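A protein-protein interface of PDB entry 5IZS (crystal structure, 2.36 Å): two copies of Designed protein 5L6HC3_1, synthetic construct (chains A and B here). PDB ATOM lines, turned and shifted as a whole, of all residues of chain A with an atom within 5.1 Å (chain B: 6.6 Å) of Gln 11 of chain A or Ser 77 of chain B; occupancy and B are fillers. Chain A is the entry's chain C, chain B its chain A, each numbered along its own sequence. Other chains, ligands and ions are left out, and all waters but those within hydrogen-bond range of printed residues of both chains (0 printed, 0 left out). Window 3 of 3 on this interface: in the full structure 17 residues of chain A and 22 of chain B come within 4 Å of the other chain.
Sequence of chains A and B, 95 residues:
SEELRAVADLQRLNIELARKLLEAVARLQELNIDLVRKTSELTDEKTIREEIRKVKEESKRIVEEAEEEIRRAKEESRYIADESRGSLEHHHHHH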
ATOM      1  N   ALA A   6       7.307  -3.943  20.767  1.00  0.00           N
ATOM      2  CA  ALA A   6       8.233  -4.748  19.989  1.00  0.00           C
ATOM      3  C   ALA A   6       9.553  -3.998  19.858  1.00  0.00           C
ATOM      4  O   ALA A   6      10.624  -4.600  19.798  1.00  0.00           O
ATOM      5  CB  ALA A   6       7.649  -5.065  18.618  1.00  0.00           C
ATOM      6  N   VAL A   7       9.465  -2.672  19.843  1.00  0.00           N
ATOM      7  CA  VAL A   7      10.631  -1.810  19.679  1.00  0.00           C
ATOM      8  C   VAL A   7      11.521  -1.811  20.923  1.00  0.00           C
ATOM      9  O   VAL A   7      12.749  -1.816  20.820  1.00  0.00           O
ATOM     10  CB  VAL A   7      10.205  -0.368  19.355  1.00  0.00           C
ATOM     11  CG1 VAL A   7      11.416   0.531  19.220  1.00  0.00           C
ATOM     12  CG2 VAL A   7       9.376  -0.342  18.079  1.00  0.00           C
ATOM     13  N   ALA A   8      10.897  -1.812  22.099  1.00  0.00           N
ATOM     14  CA  ALA A   8      11.635  -1.850  23.358  1.00  0.00           C
ATOM     15  C   ALA A   8      12.413  -3.157  23.499  1.00  0.00           C
ATOM     16  O   ALA A   8      13.501  -3.184  24.077  1.00  0.00           O
ATOM     17  CB  ALA A   8      10.690  -1.668  24.537  1.00  0.00           C
ATOM     18  N   ASP A   9      11.847  -4.235  22.963  1.00  0.00           N
ATOM     19  CA  ASP A   9      12.486  -5.546  23.007  1.00  0.00           C
ATOM     20  C   ASP A   9      13.596  -5.657  21.973  1.00  0.00           C
ATOM     21  O   ASP A   9      14.613  -6.306  22.210  1.00  0.00           O
ATOM     22  CB  ASP A   9      11.461  -6.657  22.793  1.00  0.00           C
ATOM     23  CG  ASP A   9      10.528  -6.821  23.972  1.00  0.00           C
ATOM     24  OD1 ASP A   9      10.910  -6.418  25.093  1.00  0.00           O
ATOM     25  OD2 ASP A   9       9.415  -7.353  23.780  1.00  0.00           O
ATOM     26  N   LEU A  10      13.390  -5.030  20.819  1.00  0.00           N
ATOM     27  CA  LEU A  10      14.432  -4.937  19.806  1.00  0.00           C
ATOM     28  C   LEU A  10      15.604  -4.125  20.336  1.00  0.00           C
ATOM     29  O   LEU A  10      16.766  -4.400  20.023  1.00  0.00           O
ATOM     30  CB  LEU A  10      13.883  -4.302  18.529  1.00  0.00           C
ATOM     31  CG  LEU A  10      13.164  -5.262  17.584  1.00  0.00           C
ATOM     32  CD1 LEU A  10      12.528  -4.516  16.426  1.00  0.00           C
ATOM     33  CD2 LEU A  10      14.151  -6.295  17.078  1.00  0.00           C
ATOM     34  N   GLN A  11      15.283  -3.127  21.149  1.00  0.00           N
ATOM     35  CA  GLN A  11      16.286  -2.239  21.713  1.00  0.00           C
ATOM     36  C   GLN A  11      17.215  -2.968  22.685  1.00  0.00           C
ATOM     37  O   GLN A  11      18.433  -2.807  22.616  1.00  0.00           O
ATOM     38  CB  GLN A  11      15.610  -1.060  22.413  1.00  0.00           C
ATOM     39  CG  GLN A  11      16.576  -0.003  22.912  1.00  0.00           C
ATOM     40  CD  GLN A  11      17.244   0.766  21.787  1.00  0.00           C
ATOM     41  OE1 GLN A  11      16.811   0.711  20.636  1.00  0.00           O
ATOM     42  NE2 GLN A  11      18.308   1.490  22.117  1.00  0.00           N
ATOM     43  N   ARG A  12      16.644  -3.770  23.581  1.00  0.00           N
ATOM     44  CA  ARG A  12      17.439  -4.513  24.558  1.00  0.00           C
ATOM     45  C   ARG A  12      18.313  -5.557  23.860  1.00  0.00           C
ATOM     46  O   ARG A  12      19.404  -5.881  24.328  1.00  0.00           O
ATOM     47  CB  ARG A  12      16.535  -5.176  25.606  1.00  0.00           C
ATOM     48  CG  ARG A  12      17.273  -5.659  26.852  1.00  0.00           C
ATOM     49  CD  ARG A  12      16.370  -6.447  27.807  1.00  0.00           C
ATOM     50  NE  ARG A  12      15.620  -5.602  28.734  1.00  0.00           N
ATOM     51  CZ  ARG A  12      14.293  -5.554  28.797  1.00  0.00           C
ATOM     52  NH1 ARG A  12      13.556  -6.301  27.986  1.00  0.00           N
ATOM     53  NH2 ARG A  12      13.698  -4.757  29.675  1.00  0.00           N
ATOM     54  N   LEU A  13      17.826  -6.064  22.727  1.00  0.00           N
ATOM     55  CA  LEU A  13      18.595  -6.974  21.885  1.00  0.00           C
ATOM     56  C   LEU A  13      19.882  -6.288  21.427  1.00  0.00           C
ATOM     57  O   LEU A  13      20.953  -6.890  21.441  1.00  0.00           O
ATOM     58  CB  LEU A  13      17.754  -7.428  20.684  1.00  0.00           C
ATOM     59  CG  LEU A  13      18.238  -8.579  19.797  1.00  0.00           C
ATOM     60  CD1 LEU A  13      18.674  -9.764  20.638  1.00  0.00           C
ATOM     61  CD2 LEU A  13      17.133  -8.994  18.832  1.00  0.00           C
ATOM     62  N   ASN A  14      19.776  -5.015  21.057  1.00  0.00           N
ATOM     63  CA  ASN A  14      20.937  -4.235  20.632  1.00  0.00           C
ATOM     64  C   ASN A  14      21.874  -3.894  21.793  1.00  0.00           C
ATOM     65  O   ASN A  14      23.091  -3.832  21.623  1.00  0.00           O
ATOM     66  CB  ASN A  14      20.489  -2.950  19.938  1.00  0.00           C
ATOM     67  CG  ASN A  14      19.672  -3.217  18.686  1.00  0.00           C
ATOM     68  OD1 ASN A  14      19.790  -4.274  18.064  1.00  0.00           O
ATOM     69  ND2 ASN A  14      18.839  -2.254  18.307  1.00  0.00           N
ATOM     70  N   ILE A  15      21.295  -3.672  22.972  1.00  0.00           N
ATOM     71  CA  ILE A  15      22.073  -3.426  24.183  1.00  0.00           C
ATOM     72  C   ILE A  15      22.863  -4.669  24.560  1.00  0.00           C
ATOM     73  O   ILE A  15      24.051  -4.593  24.884  1.00  0.00           O
ATOM     74  CB  ILE A  15      21.171  -3.003  25.357  1.00  0.00           C
ATOM     75  CG1 ILE A  15      20.849  -1.514  25.248  1.00  0.00           C
ATOM     76  CG2 ILE A  15      21.847  -3.284  26.695  1.00  0.00           C
ATOM     77  CD1 ILE A  15      22.074  -0.623  25.298  1.00  0.00           C
ATOM     78  N   ASP B   9      14.150   8.310  18.455  1.00  0.00           N
ATOM     79  CA  ASP B   9      14.924   8.590  19.661  1.00  0.00           C
ATOM     80  C   ASP B   9      15.778   7.396  20.075  1.00  0.00           C
ATOM     81  O   ASP B   9      16.955   7.549  20.402  1.00  0.00           O
ATOM     82  CB  ASP B   9      13.997   8.998  20.807  1.00  0.00           C
ATOM     83  CG  ASP B   9      13.492  10.422  20.664  1.00  0.00           C
ATOM     84  OD1 ASP B   9      14.228  11.256  20.094  1.00  0.00           O
ATOM     85  OD2 ASP B   9      12.364  10.709  21.115  1.00  0.00           O
ATOM     86  N   LEU B  10      15.178   6.208  20.059  1.00  0.00           N
ATOM     87  CA  LEU B  10      15.898   4.980  20.370  1.00  0.00           C
ATOM     88  C   LEU B  10      16.971   4.698  19.324  1.00  0.00           C
ATOM     89  O   LEU B  10      18.027   4.141  19.630  1.00  0.00           O
ATOM     90  CB  LEU B  10      14.929   3.800  20.464  1.00  0.00           C
ATOM     91  CG  LEU B  10      13.957   3.839  21.645  1.00  0.00           C
ATOM     92  CD1 LEU B  10      13.010   2.652  21.607  1.00  0.00           C
ATOM     93  CD2 LEU B  10      14.719   3.875  22.961  1.00  0.00           C
ATOM     94  N   GLN B  11      16.693   5.095  18.087  1.00  0.00           N
ATOM     95  CA  GLN B  11      17.622   4.888  16.988  1.00  0.00           C
ATOM     96  C   GLN B  11      18.862   5.763  17.144  1.00  0.00           C
ATOM     97  O   GLN B  11      19.986   5.322  16.897  1.00  0.00           O
ATOM     98  CB  GLN B  11      16.936   5.179  15.656  1.00  0.00           C
ATOM     99  CG  GLN B  11      17.753   4.773  14.453  1.00  0.00           C
ATOM    100  CD  GLN B  11      17.997   3.279  14.399  1.00  0.00           C
ATOM    101  OE1 GLN B  11      17.221   2.492  14.940  1.00  0.00           O
ATOM    102  NE2 GLN B  11      19.083   2.880  13.747  1.00  0.00           N
ATOM    103  N   LEU B  13      19.997   6.731  19.862  1.00  0.00           N
ATOM    104  CA  LEU B  13      20.694   6.171  21.012  1.00  0.00           C
ATOM    105  C   LEU B  13      21.697   5.104  20.579  1.00  0.00           C
ATOM    106  O   LEU B  13      22.842   5.095  21.029  1.00  0.00           O
ATOM    107  CB  LEU B  13      19.678   5.588  21.998  1.00  0.00           C
ATOM    108  CG  LEU B  13      20.138   5.321  23.427  1.00  0.00           C
ATOM    109  CD1 LEU B  13      21.048   6.439  23.877  1.00  0.00           C
ATOM    110  CD2 LEU B  13      18.934   5.207  24.348  1.00  0.00           C
ATOM    111  N   ASN B  14      21.260   4.218  19.691  1.00  0.00           N
ATOM    112  CA  ASN B  14      22.119   3.160  19.171  1.00  0.00           C
ATOM    113  C   ASN B  14      23.297   3.718  18.371  1.00  0.00           C
ATOM    114  O   ASN B  14      24.413   3.204  18.452  1.00  0.00           O
ATOM    115  CB  ASN B  14      21.304   2.196  18.307  1.00  0.00           C
ATOM    116  CG  ASN B  14      20.166   1.545  19.075  1.00  0.00           C
ATOM    117  OD1 ASN B  14      20.281   1.277  20.273  1.00  0.00           O
ATOM    118  ND2 ASN B  14      19.058   1.290  18.387  1.00  0.00           N
ATOM    119  N   LEU B  17      25.774   4.879  20.789  1.00  0.00           N
ATOM    120  CA  LEU B  17      26.446   3.724  21.370  1.00  0.00           C
ATOM    121  C   LEU B  17      27.567   3.228  20.459  1.00  0.00           C
ATOM    122  O   LEU B  17      28.708   3.095  20.894  1.00  0.00           O
ATOM    123  CB  LEU B  17      25.435   2.607  21.642  1.00  0.00           C
ATOM    124  CG  LEU B  17      25.757   1.619  22.761  1.00  0.00           C
ATOM    125  CD1 LEU B  17      26.277   2.343  23.992  1.00  0.00           C
ATOM    126  CD2 LEU B  17      24.513   0.819  23.104  1.00  0.00           C
ATOM    127  N   ARG B  72      24.242   3.022  30.671  1.00  0.00           N
ATOM    128  CA  ARG B  72      23.482   4.271  30.643  1.00  0.00           C
ATOM    129  C   ARG B  72      22.564   4.349  29.428  1.00  0.00           C
ATOM    130  O   ARG B  72      21.443   4.851  29.517  1.00  0.00           O
ATOM    131  CB  ARG B  72      24.422   5.476  30.659  1.00  0.00           C
ATOM    132  CG  ARG B  72      24.751   5.981  32.055  1.00  0.00           C
ATOM    133  CD  ARG B  72      25.287   7.404  32.012  1.00  0.00           C
ATOM    134  NE  ARG B  72      26.526   7.511  31.247  1.00  0.00           N
ATOM    135  CZ  ARG B  72      27.740   7.495  31.786  1.00  0.00           C
ATOM    136  NH1 ARG B  72      27.885   7.375  33.099  1.00  0.00           N
ATOM    137  NH2 ARG B  72      28.812   7.601  31.011  1.00  0.00           N
ATOM    138  N   ALA B  73      23.049   3.857  28.292  1.00  0.00           N
ATOM    139  CA  ALA B  73      22.230   3.771  27.090  1.00  0.00           C
ATOM    140  C   ALA B  73      21.042   2.847  27.338  1.00  0.00           C
ATOM    141  O   ALA B  73      19.931   3.109  26.878  1.00  0.00           O
ATOM    142  CB  ALA B  73      23.055   3.279  25.915  1.00  0.00           C
ATOM    143  N   LYS B  74      21.293   1.775  28.085  1.00  0.00           N
ATOM    144  CA  LYS B  74      20.278   0.781  28.415  1.00  0.00           C
ATOM    145  C   LYS B  74      19.198   1.359  29.325  1.00  0.00           C
ATOM    146  O   LYS B  74      18.006   1.131  29.115  1.00  0.00           O
ATOM    147  CB  LYS B  74      20.934  -0.432  29.077  1.00  0.00           C
ATOM    148  CG  LYS B  74      19.988  -1.559  29.454  1.00  0.00           C
ATOM    149  CD  LYS B  74      20.757  -2.694  30.121  1.00  0.00           C
ATOM    150  CE  LYS B  74      19.859  -3.883  30.427  1.00  0.00           C
ATOM    151  NZ  LYS B  74      20.633  -5.023  30.987  1.00  0.00           N
ATOM    152  N   GLU B  75      19.626   2.105  30.338  1.00  0.00           N
ATOM    153  CA  GLU B  75      18.702   2.741  31.269  1.00  0.00           C
ATOM    154  C   GLU B  75      17.882   3.816  30.559  1.00  0.00           C
ATOM    155  O   GLU B  75      16.690   3.975  30.819  1.00  0.00           O
ATOM    156  CB  GLU B  75      19.461   3.342  32.453  1.00  0.00           C
ATOM    157  CG  GLU B  75      20.139   2.312  33.349  1.00  0.00           C
ATOM    158  CD  GLU B  75      21.031   2.943  34.405  1.00  0.00           C
ATOM    159  OE1 GLU B  75      20.929   2.548  35.586  1.00  0.00           O
ATOM    160  OE2 GLU B  75      21.835   3.834  34.057  1.00  0.00           O
ATOM    161  N   GLU B  76      18.528   4.542  29.650  1.00  0.00           N
ATOM    162  CA  GLU B  76      17.858   5.590  28.889  1.00  0.00           C
ATOM    163  C   GLU B  76      16.821   4.997  27.937  1.00  0.00           C
ATOM    164  O   GLU B  76      15.790   5.611  27.676  1.00  0.00           O
ATOM    165  CB  GLU B  76      18.878   6.424  28.110  1.00  0.00           C
ATOM    166  CG  GLU B  76      18.284   7.615  27.363  1.00  0.00           C
ATOM    167  CD  GLU B  76      17.731   8.686  28.290  1.00  0.00           C
ATOM    168  OE1 GLU B  76      18.044   8.666  29.500  1.00  0.00           O
ATOM    169  OE2 GLU B  76      16.975   9.553  27.805  1.00  0.00           O
ATOM    170  N   SER B  77      17.099   3.801  27.425  1.00  0.00           N
ATOM    171  CA  SER B  77      16.147   3.098  26.567  1.00  0.00           C
ATOM    172  C   SER B  77      14.890   2.736  27.347  1.00  0.00           C
ATOM    173  O   SER B  77      13.777   2.824  26.831  1.00  0.00           O
ATOM    174  CB  SER B  77      16.780   1.838  25.977  1.00  0.00           C
ATOM    175  OG  SER B  77      17.708   2.169  24.956  1.00  0.00           O
ATOM    176  N   ARG B  78      15.090   2.333  28.597  1.00  0.00           N
ATOM    177  CA  ARG B  78      13.998   1.979  29.495  1.00  0.00           C
ATOM    178  C   ARG B  78      13.075   3.165  29.782  1.00  0.00           C
ATOM    179  O   ARG B  78      11.852   3.016  29.809  1.00  0.00           O
ATOM    180  CB  ARG B  78      14.561   1.415  30.803  1.00  0.00           C
ATOM    181  CG  ARG B  78      13.703   1.690  32.026  1.00  0.00           C
ATOM    182  CD  ARG B  78      14.135   0.867  33.237  1.00  0.00           C
ATOM    183  NE  ARG B  78      15.132   1.538  34.070  1.00  0.00           N
ATOM    184  CZ  ARG B  78      16.404   1.163  34.167  1.00  0.00           C
ATOM    185  NH1 ARG B  78      16.845   0.120  33.477  1.00  0.00           N
ATOM    186  NH2 ARG B  78      17.237   1.830  34.956  1.00  0.00           N
ATOM    187  N   TYR B  79      13.658   4.342  29.993  1.00  0.00           N
ATOM    188  CA  TYR B  79      12.860   5.540  30.228  1.00  0.00           C
ATOM    189  C   TYR B  79      12.076   5.926  28.979  1.00  0.00           C
ATOM    190  O   TYR B  79      10.901   6.285  29.054  1.00  0.00           O
ATOM    191  CB  TYR B  79      13.742   6.708  30.666  1.00  0.00           C
ATOM    192  CG  TYR B  79      13.007   8.031  30.677  1.00  0.00           C
ATOM    193  CD1 TYR B  79      13.016   8.866  29.565  1.00  0.00           C
ATOM    194  CD2 TYR B  79      12.293   8.438  31.794  1.00  0.00           C
ATOM    195  CE1 TYR B  79      12.336  10.069  29.567  1.00  0.00           C
ATOM    196  CE2 TYR B  79      11.613   9.642  31.807  1.00  0.00           C
ATOM    197  CZ  TYR B  79      11.638  10.454  30.692  1.00  0.00           C
ATOM    198  OH  TYR B  79      10.959  11.654  30.705  1.00  0.00           O
ATOM    199  N   ILE B  80      12.739   5.868  27.832  1.00  0.00           N
ATOM    200  CA  ILE B  80      12.100   6.200  26.567  1.00  0.00           C
ATOM    201  C   ILE B  80      11.013   5.162  26.264  1.00  0.00           C
ATOM    202  O   ILE B  80      10.043   5.448  25.561  1.00  0.00           O
ATOM    203  CB  ILE B  80      13.143   6.287  25.427  1.00  0.00           C
ATOM    204  CG1 ILE B  80      14.141   7.414  25.711  1.00  0.00           C
ATOM    205  CG2 ILE B  80      12.479   6.550  24.091  1.00  0.00           C
ATOM    206  CD1 ILE B  80      15.305   7.473  24.743  1.00  0.00           C
ATOM    207  N   ALA B  81      11.167   3.967  26.830  1.00  0.00           N
ATOM    208  CA  ALA B  81      10.159   2.914  26.727  1.00  0.00           C
ATOM    209  C   ALA B  81       8.977   3.189  27.645  1.00  0.00           C
ATOM    210  O   ALA B  81       7.876   2.716  27.390  1.00  0.00           O
ATOM    211  CB  ALA B  81      10.770   1.559  27.064  1.00  0.00           C
ATOM    212  N   ASP B  82       9.248   3.973  28.688  1.00  0.00           N
ATOM    213  CA  ASP B  82       8.396   4.237  29.863  1.00  0.00           C
ATOM    214  C   ASP B  82       8.375   3.024  30.795  1.00  0.00           C
ATOM    215  O   ASP B  82       9.373   2.723  31.453  1.00  0.00           O
ATOM    216  CB  ASP B  82       6.961   4.705  29.476  1.00  0.00           C
ATOM    217  CG  ASP B  82       5.979   3.563  29.121  1.00  0.00           C
ATOM    218  OD1 ASP B  82       6.129   2.398  29.552  1.00  0.00           O
ATOM    219  OD2 ASP B  82       5.012   3.854  28.386  1.00  0.00           O
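The backbone carbonyl oxygen (O) of Leu 10 of chain B is in hydrogen-bond range of the side-chain amide nitrogen (ND2) of Asn 14 of chain B.
The backbone carbonyl oxygen (O) of Ala 73 of chain B lies within hydrogen-bond range of the side-chain hydroxyl (OG) of Ser 77 of chain B (3.1 Å).
O of Leu 10 of chain A lies close to ND2 of Asn 14 of chain A (3.4 Å).
Of chain B, only Leu 10, Asn 14 and Ser 77 come within 4 Å of Gln 11 of chain A.
Leu 13 of chain A touches none of the printed residues of chain B.
Of the printed residues of chain B, Ile 15 of chain A touches Leu 17 and Lys 74.
Of the printed residues of chain A, Lys 74 of chain B touches Ile 15 (3.6 Å).
Ser 77 of chain B touches one residue of chain A.
The nearest residue of chain A that does not touch Ser 77 of chain B is Ile 15 of chain A (4.8 Å).
Among the printed residues, merely in contact across the chains: Val 7 of chain A with Leu 10 of chain B (3.6 Å), Gln 11 of chain A with Leu 10 of chain B (3.6 Å), Asn 14 of chain A with Asn 14 of chain B (3.6 Å), Ile 15 of chain A with Leu 17 of chain B (3.6 Å) and Ile 15 of chain A with Lys 74 of chain B (3.6 Å).
OD1 of Asn 14 of chain B sits at hydrogen-bond distance from NE2 of Gln 11 of chain A, at 2.7 Å.
The side-chain hydroxyl of Ser 77 of chain B sits at hydrogen-bond distance from the side-chain amide nitrogen of Gln 11 of chain A.
Gln 11 of chain A touches Leu 10 of chain B, but with the chains exchanged Leu 10 of chain A does not touch Gln 11 of chain B (8.4 Å).
Gln 11 of chain A touches Asn 14 of chain B, but with the chains exchanged Asn 14 of chain A does not touch Gln 11 of chain B (6.0 Å).
Asn 14 of chain A touches its own counterpart, Asn 14 of chain B.
Positions printed for both chains: 9, 10, 11, 13 and 14.
Printed residues of chain A that touch a printed residue of chain B: Val 7, Gln 11, Asn 14 and Ile 15.
Hydrophobic or aromatic side chains of chain B within 4 Å of the printed part of chain A: Leu 10 and Leu 17.
Among the printed residues, 7 pairs touch across the chains.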
